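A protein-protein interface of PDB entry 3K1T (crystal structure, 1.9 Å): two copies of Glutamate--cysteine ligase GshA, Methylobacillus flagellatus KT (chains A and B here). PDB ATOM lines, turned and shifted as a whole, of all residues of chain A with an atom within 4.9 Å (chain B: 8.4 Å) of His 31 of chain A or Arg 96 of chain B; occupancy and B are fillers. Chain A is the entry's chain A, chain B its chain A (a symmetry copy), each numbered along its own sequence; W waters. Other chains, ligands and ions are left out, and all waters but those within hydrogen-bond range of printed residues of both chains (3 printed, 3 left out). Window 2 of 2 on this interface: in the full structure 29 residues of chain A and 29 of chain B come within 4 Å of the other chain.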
ATOM      1  N   PRO A  27      33.192  22.803  28.228  1.00  0.00           N
ATOM      2  CA  PRO A  27      31.733  22.708  28.094  1.00  0.00           C
ATOM      3  C   PRO A  27      30.942  23.257  29.306  1.00  0.00           C
ATOM      4  O   PRO A  27      29.875  23.855  29.137  1.00  0.00           O
ATOM      5  CB  PRO A  27      31.475  21.206  27.924  1.00  0.00           C
ATOM      6  CG  PRO A  27      32.831  20.505  27.979  1.00  0.00           C
ATOM      7  CD  PRO A  27      33.891  21.513  28.018  1.00  0.00           C
ATOM      8  N   ARG A  28      31.447  23.050  30.521  1.00  0.00           N
ATOM      9  CA  ARG A  28      30.794  23.623  31.699  1.00  0.00           C
ATOM     10  C   ARG A  28      30.721  25.135  31.626  1.00  0.00           C
ATOM     11  O   ARG A  28      29.673  25.734  31.958  1.00  0.00           O
ATOM     12  CB  ARG A  28      31.466  23.163  33.013  1.00  0.00           C
ATOM     13  CG  ARG A  28      31.479  24.191  34.143  1.00  0.00           C
ATOM     14  CD  ARG A  28      32.360  23.763  35.336  1.00  0.00           C
ATOM     15  NE  ARG A  28      31.605  22.893  36.213  1.00  0.00           N
ATOM     16  CZ  ARG A  28      31.463  21.583  36.051  1.00  0.00           C
ATOM     17  NH1 ARG A  28      32.079  20.938  35.066  1.00  0.00           N
ATOM     18  NH2 ARG A  28      30.723  20.903  36.913  1.00  0.00           N
ATOM     19  N   ILE A  29      31.807  25.759  31.203  1.00  0.00           N
ATOM     20  CA  ILE A  29      31.869  27.206  31.026  1.00  0.00           C
ATOM     21  C   ILE A  29      30.869  27.706  29.974  1.00  0.00           C
ATOM     22  O   ILE A  29      30.132  28.664  30.216  1.00  0.00           O
ATOM     23  CB  ILE A  29      33.299  27.659  30.686  1.00  0.00           C
ATOM     24  CG1 ILE A  29      34.224  27.486  31.922  1.00  0.00           C
ATOM     25  CG2 ILE A  29      33.345  29.142  30.111  1.00  0.00           C
ATOM     26  CD1 ILE A  29      35.710  27.467  31.542  1.00  0.00           C
ATOM     27  N   GLU A  30      30.845  27.072  28.805  1.00  0.00           N
ATOM     28  CA  GLU A  30      29.951  27.508  27.746  1.00  0.00           C
ATOM     29  C   GLU A  30      28.458  27.295  28.130  1.00  0.00           C
ATOM     30  O   GLU A  30      27.600  28.156  27.856  1.00  0.00           O
ATOM     31  CB  GLU A  30      30.304  26.826  26.431  1.00  0.00           C
ATOM     32  CG  GLU A  30      31.711  27.178  25.957  1.00  0.00           C
ATOM     33  CD  GLU A  30      31.932  28.659  25.670  1.00  0.00           C
ATOM     34  OE1 GLU A  30      30.952  29.427  25.495  1.00  0.00           O
ATOM     35  OE2 GLU A  30      33.115  29.066  25.630  1.00  0.00           O
ATOM     36  N   HIS A  31      28.166  26.188  28.797  1.00  0.00           N
ATOM     37  CA  HIS A  31      26.827  25.961  29.335  1.00  0.00           C
ATOM     38  C   HIS A  31      26.462  27.030  30.361  1.00  0.00           C
ATOM     39  O   HIS A  31      25.357  27.582  30.334  1.00  0.00           O
ATOM     40  CB  HIS A  31      26.729  24.578  29.987  1.00  0.00           C
ATOM     41  CG  HIS A  31      25.408  24.327  30.614  1.00  0.00           C
ATOM     42  ND1 HIS A  31      25.181  24.497  31.962  1.00  0.00           N
ATOM     43  CD2 HIS A  31      24.212  24.021  30.062  1.00  0.00           C
ATOM     44  CE1 HIS A  31      23.912  24.232  32.222  1.00  0.00           C
ATOM     45  NE2 HIS A  31      23.304  23.934  31.092  1.00  0.00           N
ATOM     46  N   TRP A  32      27.418  27.392  31.224  1.00  0.00           N
ATOM     47  CA  TRP A  32      27.158  28.438  32.222  1.00  0.00           C
ATOM     48  C   TRP A  32      26.857  29.777  31.542  1.00  0.00           C
ATOM     49  O   TRP A  32      25.891  30.457  31.899  1.00  0.00           O
ATOM     50  CB  TRP A  32      28.346  28.536  33.185  1.00  0.00           C
ATOM     51  CG  TRP A  32      28.191  29.569  34.266  1.00  0.00           C
ATOM     52  CD1 TRP A  32      27.613  29.389  35.485  1.00  0.00           C
ATOM     53  CD2 TRP A  32      28.652  30.921  34.234  1.00  0.00           C
ATOM     54  NE1 TRP A  32      27.674  30.534  36.212  1.00  0.00           N
ATOM     55  CE2 TRP A  32      28.300  31.504  35.471  1.00  0.00           C
ATOM     56  CE3 TRP A  32      29.316  31.699  33.284  1.00  0.00           C
ATOM     57  CZ2 TRP A  32      28.604  32.824  35.790  1.00  0.00           C
ATOM     58  CZ3 TRP A  32      29.644  32.994  33.608  1.00  0.00           C
ATOM     59  CH2 TRP A  32      29.278  33.552  34.861  1.00  0.00           C
ATOM     60  N   PHE A  33      27.649  30.160  30.546  1.00  0.00           N
ATOM     61  CA  PHE A  33      27.376  31.419  29.849  1.00  0.00           C
ATOM     62  C   PHE A  33      25.990  31.393  29.216  1.00  0.00           C
ATOM     63  O   PHE A  33      25.234  32.370  29.309  1.00  0.00           O
ATOM     64  CB  PHE A  33      28.419  31.687  28.755  1.00  0.00           C
ATOM     65  CG  PHE A  33      29.665  32.412  29.228  1.00  0.00           C
ATOM     66  CD1 PHE A  33      29.585  33.694  29.756  1.00  0.00           C
ATOM     67  CD2 PHE A  33      30.918  31.811  29.114  1.00  0.00           C
ATOM     68  CE1 PHE A  33      30.715  34.364  30.173  1.00  0.00           C
ATOM     69  CE2 PHE A  33      32.072  32.494  29.513  1.00  0.00           C
ATOM     70  CZ  PHE A  33      31.952  33.771  30.045  1.00  0.00           C
ATOM     71  N   ARG A  34      25.634  30.290  28.556  1.00  0.00           N
ATOM     72  CA  ARG A  34      24.282  30.206  27.979  1.00  0.00           C
ATOM     73  C   ARG A  34      23.188  30.408  29.028  1.00  0.00           C
ATOM     74  O   ARG A  34      22.216  31.132  28.739  1.00  0.00           O
ATOM     75  CB  ARG A  34      24.048  28.905  27.205  1.00  0.00           C
ATOM     76  CG  ARG A  34      24.664  28.975  25.807  1.00  0.00           C
ATOM     77  CD  ARG A  34      24.265  27.746  24.989  1.00  0.00           C
ATOM     78  NE  ARG A  34      25.002  26.544  25.303  1.00  0.00           N
ATOM     79  CZ  ARG A  34      26.131  26.192  24.668  1.00  0.00           C
ATOM     80  NH1 ARG A  34      26.656  26.954  23.706  1.00  0.00           N
ATOM     81  NH2 ARG A  34      26.718  25.089  25.007  1.00  0.00           N
ATOM     82  N   SER A  35      23.334  29.814  30.225  1.00  0.00           N
ATOM     83  CA  SER A  35      22.375  30.074  31.292  1.00  0.00           C
ATOM     84  C   SER A  35      22.324  31.571  31.642  1.00  0.00           C
ATOM     85  O   SER A  35      21.236  32.109  31.858  1.00  0.00           O
ATOM     86  CB  SER A  35      22.689  29.271  32.555  1.00  0.00           C
ATOM     87  OG  SER A  35      22.638  27.911  32.223  1.00  0.00           O
ATOM     88  N   MET B  85      26.348  27.411  17.842  1.00  0.00           N
ATOM     89  CA  MET B  85      25.903  27.949  19.145  1.00  0.00           C
ATOM     90  C   MET B  85      24.518  28.583  19.128  1.00  0.00           C
ATOM     91  O   MET B  85      23.713  28.359  20.035  1.00  0.00           O
ATOM     92  CB  MET B  85      26.901  28.960  19.729  1.00  0.00           C
ATOM     93  CG  MET B  85      28.121  28.288  20.225  1.00  0.00           C
ATOM     94  SD  MET B  85      29.434  29.640  20.817  1.00  0.00           S
ATOM     95  CE  MET B  85      30.333  28.510  22.180  1.00  0.00           C
ATOM     96  N   VAL B  88      22.061  25.625  18.958  1.00  0.00           N
ATOM     97  CA  VAL B  88      21.914  25.093  20.314  1.00  0.00           C
ATOM     98  C   VAL B  88      20.994  25.960  21.188  1.00  0.00           C
ATOM     99  O   VAL B  88      20.111  25.433  21.882  1.00  0.00           O
ATOM    100  CB  VAL B  88      23.275  24.910  20.975  1.00  0.00           C
ATOM    101  CG1 VAL B  88      23.139  24.640  22.527  1.00  0.00           C
ATOM    102  CG2 VAL B  88      24.070  23.814  20.243  1.00  0.00           C
ATOM    103  N   CYS B  92      17.998  23.491  21.568  1.00  0.00           N
ATOM    104  CA  CYS B  92      18.193  22.735  22.821  1.00  0.00           C
ATOM    105  C   CYS B  92      18.934  23.602  23.862  1.00  0.00           C
ATOM    106  O   CYS B  92      20.074  23.319  24.244  1.00  0.00           O
ATOM    107  CB  CYS B  92      18.894  21.389  22.541  1.00  0.00           C
ATOM    108  SG  CYS B  92      20.402  21.470  21.585  1.00  0.00           S
ATOM    109  N   PRO B  93      18.260  24.667  24.340  1.00  0.00           N
ATOM    110  CA  PRO B  93      18.964  25.738  25.043  1.00  0.00           C
ATOM    111  C   PRO B  93      19.684  25.340  26.302  1.00  0.00           C
ATOM    112  O   PRO B  93      20.672  25.990  26.658  1.00  0.00           O
ATOM    113  CB  PRO B  93      17.850  26.766  25.360  1.00  0.00           C
ATOM    114  CG  PRO B  93      16.572  26.077  25.127  1.00  0.00           C
ATOM    115  CD  PRO B  93      16.862  25.030  24.070  1.00  0.00           C
ATOM    116  N   ASP B  94      19.189  24.302  26.976  1.00  0.00           N
ATOM    117  CA  ASP B  94      19.699  23.929  28.273  1.00  0.00           C
ATOM    118  C   ASP B  94      20.612  22.702  28.215  1.00  0.00           C
ATOM    119  O   ASP B  94      21.093  22.237  29.257  1.00  0.00           O
ATOM    120  CB  ASP B  94      18.512  23.656  29.184  1.00  0.00           C
ATOM    121  CG  ASP B  94      17.610  24.886  29.327  1.00  0.00           C
ATOM    122  OD1 ASP B  94      18.167  25.995  29.573  1.00  0.00           O
ATOM    123  OD2 ASP B  94      16.366  24.739  29.173  1.00  0.00           O
ATOM    124  N   ALA B  95      20.835  22.201  27.001  1.00  0.00           N
ATOM    125  CA  ALA B  95      21.639  21.011  26.789  1.00  0.00           C
ATOM    126  C   ALA B  95      23.068  21.181  27.288  1.00  0.00           C
ATOM    127  O   ALA B  95      23.701  22.193  27.089  1.00  0.00           O
ATOM    128  CB  ALA B  95      21.638  20.606  25.299  1.00  0.00           C
ATOM    129  N   ARG B  96      23.536  20.193  28.027  1.00  0.00           N
ATOM    130  CA  ARG B  96      24.947  20.074  28.343  1.00  0.00           C
ATOM    131  C   ARG B  96      25.583  19.019  27.440  1.00  0.00           C
ATOM    132  O   ARG B  96      26.746  19.152  27.072  1.00  0.00           O
ATOM    133  CB  ARG B  96      25.137  19.603  29.792  1.00  0.00           C
ATOM    134  CG  ARG B  96      24.708  20.565  30.852  1.00  0.00           C
ATOM    135  CD  ARG B  96      24.947  19.946  32.225  1.00  0.00           C
ATOM    136  NE  ARG B  96      24.898  20.917  33.320  1.00  0.00           N
ATOM    137  CZ  ARG B  96      23.783  21.303  33.949  1.00  0.00           C
ATOM    138  NH1 ARG B  96      22.583  20.834  33.582  1.00  0.00           N
ATOM    139  NH2 ARG B  96      23.852  22.183  34.948  1.00  0.00           N
ATOM    140  N   ARG B  97      24.830  17.946  27.174  1.00  0.00           N
ATOM    141  CA  ARG B  97      25.340  16.756  26.494  1.00  0.00           C
ATOM    142  C   ARG B  97      24.511  16.470  25.238  1.00  0.00           C
ATOM    143  O   ARG B  97      23.303  16.674  25.241  1.00  0.00           O
ATOM    144  CB  ARG B  97      25.256  15.551  27.439  1.00  0.00           C
ATOM    145  CG  ARG B  97      26.209  15.610  28.629  1.00  0.00           C
ATOM    146  CD  ARG B  97      25.972  14.483  29.620  1.00  0.00           C
ATOM    147  NE  ARG B  97      24.749  14.686  30.397  1.00  0.00           N
ATOM    148  CZ  ARG B  97      24.633  15.506  31.455  1.00  0.00           C
ATOM    149  NH1 ARG B  97      25.660  16.241  31.882  1.00  0.00           N
ATOM    150  NH2 ARG B  97      23.464  15.612  32.079  1.00  0.00           N
ATOM    151  N   LEU B  98      25.151  15.980  24.187  1.00  0.00           N
ATOM    152  CA  LEU B  98      24.459  15.642  22.959  1.00  0.00           C
ATOM    153  C   LEU B  98      24.912  14.291  22.465  1.00  0.00           C
ATOM    154  O   LEU B  98      26.125  14.044  22.342  1.00  0.00           O
ATOM    155  CB  LEU B  98      24.758  16.712  21.916  1.00  0.00           C
ATOM    156  CG  LEU B  98      23.951  16.676  20.635  1.00  0.00           C
ATOM    157  CD1 LEU B  98      22.464  16.934  20.868  1.00  0.00           C
ATOM    158  CD2 LEU B  98      24.550  17.764  19.640  1.00  0.00           C
ATOM    159  N   LEU B  99      23.950  13.395  22.218  1.00  0.00           N
ATOM    160  CA  LEU B  99      24.226  12.111  21.596  1.00  0.00           C
ATOM    161  C   LEU B  99      24.044  12.280  20.103  1.00  0.00           C
ATOM    162  O   LEU B  99      22.973  12.714  19.659  1.00  0.00           O
ATOM    163  CB  LEU B  99      23.241  11.027  22.120  1.00  0.00           C
ATOM    164  CG  LEU B  99      23.438   9.591  21.622  1.00  0.00           C
ATOM    165  CD1 LEU B  99      24.704   8.985  22.217  1.00  0.00           C
ATOM    166  CD2 LEU B  99      22.213   8.691  21.956  1.00  0.00           C
ATOM    167  N   LEU B 122      30.550  20.728  17.149  1.00  0.00           N
ATOM    168  CA  LEU B 122      29.605  20.665  18.254  1.00  0.00           C
ATOM    169  C   LEU B 122      30.322  20.791  19.618  1.00  0.00           C
ATOM    170  O   LEU B 122      29.788  21.417  20.523  1.00  0.00           O
ATOM    171  CB  LEU B 122      28.797  19.362  18.189  1.00  0.00           C
ATOM    172  CG  LEU B 122      27.899  19.184  16.947  1.00  0.00           C
ATOM    173  CD1 LEU B 122      27.414  17.727  16.834  1.00  0.00           C
ATOM    174  CD2 LEU B 122      26.729  20.135  16.956  1.00  0.00           C
ATOM    175  N   ARG B 123      31.520  20.218  19.745  1.00  0.00           N
ATOM    176  CA  ARG B 123      32.332  20.363  20.953  1.00  0.00           C
ATOM    177  C   ARG B 123      32.806  21.812  21.130  1.00  0.00           C
ATOM    178  O   ARG B 123      32.822  22.344  22.263  1.00  0.00           O
ATOM    179  CB  ARG B 123      33.546  19.420  20.934  1.00  0.00           C
ATOM    180  CG  ARG B 123      33.103  17.943  21.175  1.00  0.00           C
ATOM    181  CD  ARG B 123      34.271  16.975  21.174  1.00  0.00           C
ATOM    182  NE  ARG B 123      33.752  15.629  21.441  1.00  0.00           N
ATOM    183  CZ  ARG B 123      34.264  14.490  20.988  1.00  0.00           C
ATOM    184  NH1 ARG B 123      35.347  14.486  20.225  1.00  0.00           N
ATOM    185  NH2 ARG B 123      33.681  13.327  21.321  1.00  0.00           N
ATOM    186  N   ALA B 125      31.249  24.314  20.130  1.00  0.00           N
ATOM    187  CA  ALA B 125      30.046  25.021  20.544  1.00  0.00           C
ATOM    188  C   ALA B 125      29.729  24.824  22.011  1.00  0.00           C
ATOM    189  O   ALA B 125      28.792  25.420  22.524  1.00  0.00           O
ATOM    190  CB  ALA B 125      28.813  24.637  19.620  1.00  0.00           C
ATOM    191  N   GLY B 126      30.532  24.030  22.698  1.00  0.00           N
ATOM    192  CA  GLY B 126      30.423  23.875  24.138  1.00  0.00           C
ATOM    193  C   GLY B 126      29.575  22.703  24.623  1.00  0.00           C
ATOM    194  O   GLY B 126      29.117  22.710  25.747  1.00  0.00           O
ATOM    195  N   LEU B 127      29.324  21.746  23.744  1.00  0.00           N
ATOM    196  CA  LEU B 127      28.613  20.528  24.132  1.00  0.00           C
ATOM    197  C   LEU B 127      29.587  19.376  24.412  1.00  0.00           C
ATOM    198  O   LEU B 127      30.648  19.277  23.806  1.00  0.00           O
ATOM    199  CB  LEU B 127      27.646  20.153  23.032  1.00  0.00           C
ATOM    200  CG  LEU B 127      26.477  21.103  22.807  1.00  0.00           C
ATOM    201  CD1 LEU B 127      25.817  20.747  21.479  1.00  0.00           C
ATOM    202  CD2 LEU B 127      25.466  21.031  24.000  1.00  0.00           C
ATOM    203  N   GLU B 128      29.223  18.515  25.369  1.00  0.00           N
ATOM    204  CA  GLU B 128      29.884  17.223  25.533  1.00  0.00           C
ATOM    205  C   GLU B 128      29.178  16.293  24.562  1.00  0.00           C
ATOM    206  O   GLU B 128      27.956  16.129  24.649  1.00  0.00           O
ATOM    207  CB  GLU B 128      29.753  16.786  26.999  1.00  0.00           C
ATOM    208  CG  GLU B 128      30.451  15.515  27.359  1.00  0.00           C
ATOM    209  CD  GLU B 128      30.112  15.044  28.808  1.00  0.00           C
ATOM    210  OE1 GLU B 128      29.771  15.925  29.668  1.00  0.00           O
ATOM    211  OE2 GLU B 128      30.169  13.801  29.044  1.00  0.00           O
ATOM    212  N   VAL B 129      29.915  15.701  23.620  1.00  0.00           N
ATOM    213  CA  VAL B 129      29.291  14.958  22.498  1.00  0.00           C
ATOM    214  C   VAL B 129      29.867  13.549  22.495  1.00  0.00           C
ATOM    215  O   VAL B 129      31.070  13.389  22.666  1.00  0.00           O
ATOM    216  CB  VAL B 129      29.621  15.600  21.136  1.00  0.00           C
ATOM    217  CG1 VAL B 129      28.978  14.807  19.958  1.00  0.00           C
ATOM    218  CG2 VAL B 129      29.194  17.070  21.130  1.00  0.00           C
ATOM    219  N   PHE B 169      26.793   8.244  30.400  1.00  0.00           N
ATOM    220  CA  PHE B 169      26.464   9.349  29.498  1.00  0.00           C
ATOM    221  C   PHE B 169      24.975   9.352  29.199  1.00  0.00           C
ATOM    222  O   PHE B 169      24.470   8.488  28.465  1.00  0.00           O
ATOM    223  CB  PHE B 169      27.222   9.244  28.181  1.00  0.00           C
ATOM    224  CG  PHE B 169      27.033  10.445  27.268  1.00  0.00           C
ATOM    225  CD1 PHE B 169      27.766  11.609  27.482  1.00  0.00           C
ATOM    226  CD2 PHE B 169      26.152  10.394  26.205  1.00  0.00           C
ATOM    227  CE1 PHE B 169      27.635  12.712  26.640  1.00  0.00           C
ATOM    228  CE2 PHE B 169      26.005  11.496  25.351  1.00  0.00           C
ATOM    229  CZ  PHE B 169      26.745  12.652  25.569  1.00  0.00           C
ATOM    230  N   ASP B 170      24.283  10.316  29.767  1.00  0.00           N
ATOM    231  CA  ASP B 170      22.861  10.448  29.489  1.00  0.00           C
ATOM    232  C   ASP B 170      22.597  11.817  28.924  1.00  0.00           C
ATOM    233  O   ASP B 170      22.676  12.800  29.648  1.00  0.00           O
ATOM    234  CB  ASP B 170      21.996  10.237  30.724  1.00  0.00           C
ATOM    235  CG  ASP B 170      20.506  10.403  30.380  1.00  0.00           C
ATOM    236  OD1 ASP B 170      20.021  11.538  30.254  1.00  0.00           O
ATOM    237  OD2 ASP B 170      19.832   9.411  30.158  1.00  0.00           O
ATOM    238  N   SER B 171      22.270  11.890  27.629  1.00  0.00           N
ATOM    239  CA  SER B 171      22.118  13.184  27.009  1.00  0.00           C
ATOM    240  C   SER B 171      20.758  13.730  27.148  1.00  0.00           C
ATOM    241  O   SER B 171      19.743  13.037  27.307  1.00  0.00           O
ATOM    242  CB  SER B 171      22.479  13.169  25.517  1.00  0.00           C
ATOM    243  OG  SER B 171      21.587  12.343  24.796  1.00  0.00           O
ATOM    244  N   CYS B 172      20.756  15.023  26.960  1.00  0.00           N
ATOM    245  CA  CYS B 172      19.619  15.855  27.028  1.00  0.00           C
ATOM    246  C   CYS B 172      18.787  15.681  25.671  1.00  0.00           C
ATOM    247  O   CYS B 172      17.555  15.532  25.626  1.00  0.00           O
ATOM    248  CB  CYS B 172      20.242  17.281  27.341  1.00  0.00           C
ATOM    249  SG  CYS B 172      21.810  17.393  28.678  1.00  0.00           S
ATOM    250  N   ALA B 173      19.515  15.678  24.572  1.00  0.00           N
ATOM    251  CA  ALA B 173      18.936  15.602  23.256  1.00  0.00           C
ATOM    252  C   ALA B 173      19.766  14.690  22.368  1.00  0.00           C
ATOM    253  O   ALA B 173      20.900  14.341  22.701  1.00  0.00           O
ATOM    254  CB  ALA B 173      18.864  17.008  22.648  1.00  0.00           C
HETATM  255  O   HOH W   1      23.167  25.236  27.118  1.00  0.00           O
HETATM  256  O   HOH W   2      22.315  26.749  29.557  1.00  0.00           O
HETATM  257  O   HOH W   3      26.003  23.517  26.801  1.00  0.00           O
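Of the 22 printed residues of chain B, 7 touch a printed residue of chain A.
Of the 9 printed residues of chain A, 4 touch a printed residue of chain B.
Along chain A the printed residues that touch a printed residue of chain B span positions 27 to 34.
Among the printed residues, 9 pairs touch across the chains.
Among the printed residues, no Asp or Glu carboxylate lies within 4 Å of a Lys or Arg side-chain nitrogen of the other chain.
The backbone NH (N) of Arg 96 of chain B lies within hydrogen-bond range of the side-chain sulfur (SG) of Cys 172 of chain B (3.4 Å).
O of Arg 96 of chain B is in hydrogen-bond range of N of Glu 128 of chain B, 3.1 Å away.
The backbone carbonyl oxygen (O) of His 31 of chain A is in hydrogen-bond range of the side-chain hydroxyl (OG) of Ser 35 of chain A (3.3 Å).
His 31 of chain A touches three residues of chain B.
Printed residues of chain A within 4 Å of Met 85 of chain B: Glu 30.
Of the printed residues of chain A, Ala 95 of chain B touches His 31 (3.5 Å).
Of the printed residues of chain A, Ala 125 of chain B touches Arg 34 (2.9 Å).
Of the printed residues of chain A, Gly 126 of chain B touches Pro 27 (3.5 Å), Glu 30 (3.7 Å) and Arg 34 (3.5 Å).
The nearest residue of chain B that does not touch His 31 of chain A is Gly 126 of chain B (4.7 Å).
No position is printed for both chains.
Of the 9 pairs that touch across the chains among the printed residues, none has its exchanged pair printed and touching as well.
Water W3 lies within hydrogen-bond range of NH2 of Arg 34 of chain A (2.5 Å), O of Ala 95 of chain B (2.7 Å) and O of Gly 126 of chain B (3.4 Å).
Water W1 lies within hydrogen-bond range of the backbone carbonyl oxygen (O) of Pro 93 of chain B, the guanidinium group (NE) of Arg 34 of chain A and the backbone carbonyl oxygen (O) of Ala 95 of chain B.
Water W2 lies within hydrogen-bond range of OG of Ser 35 of chain A (2.9 Å), O of His 31 of chain A (3.2 Å) and O of Pro 93 of chain B (3.4 Å).
O of Asp 94 of chain B sits at hydrogen-bond distance from NE2 of His 31 of chain A.
NH2 of Arg 34 of chain A sits at hydrogen-bond distance from O of Gly 126 of chain B (3.5 Å).
NH1 of Arg 34 of chain A sits at hydrogen-bond distance from O of Ala 125 of chain B.
Among the printed residues, pairs that only touch across the chains: Pro 27 of chain A with Gly 126 of chain B, Glu 30 of chain A with Met 85 of chain B, Glu 30 of chain A with Gly 126 of chain B, His 31 of chain A with Ala 95 of chain B, His 31 of chain A with Arg 96 of chain B and Arg 34 of chain A with Val 88 of chain B.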
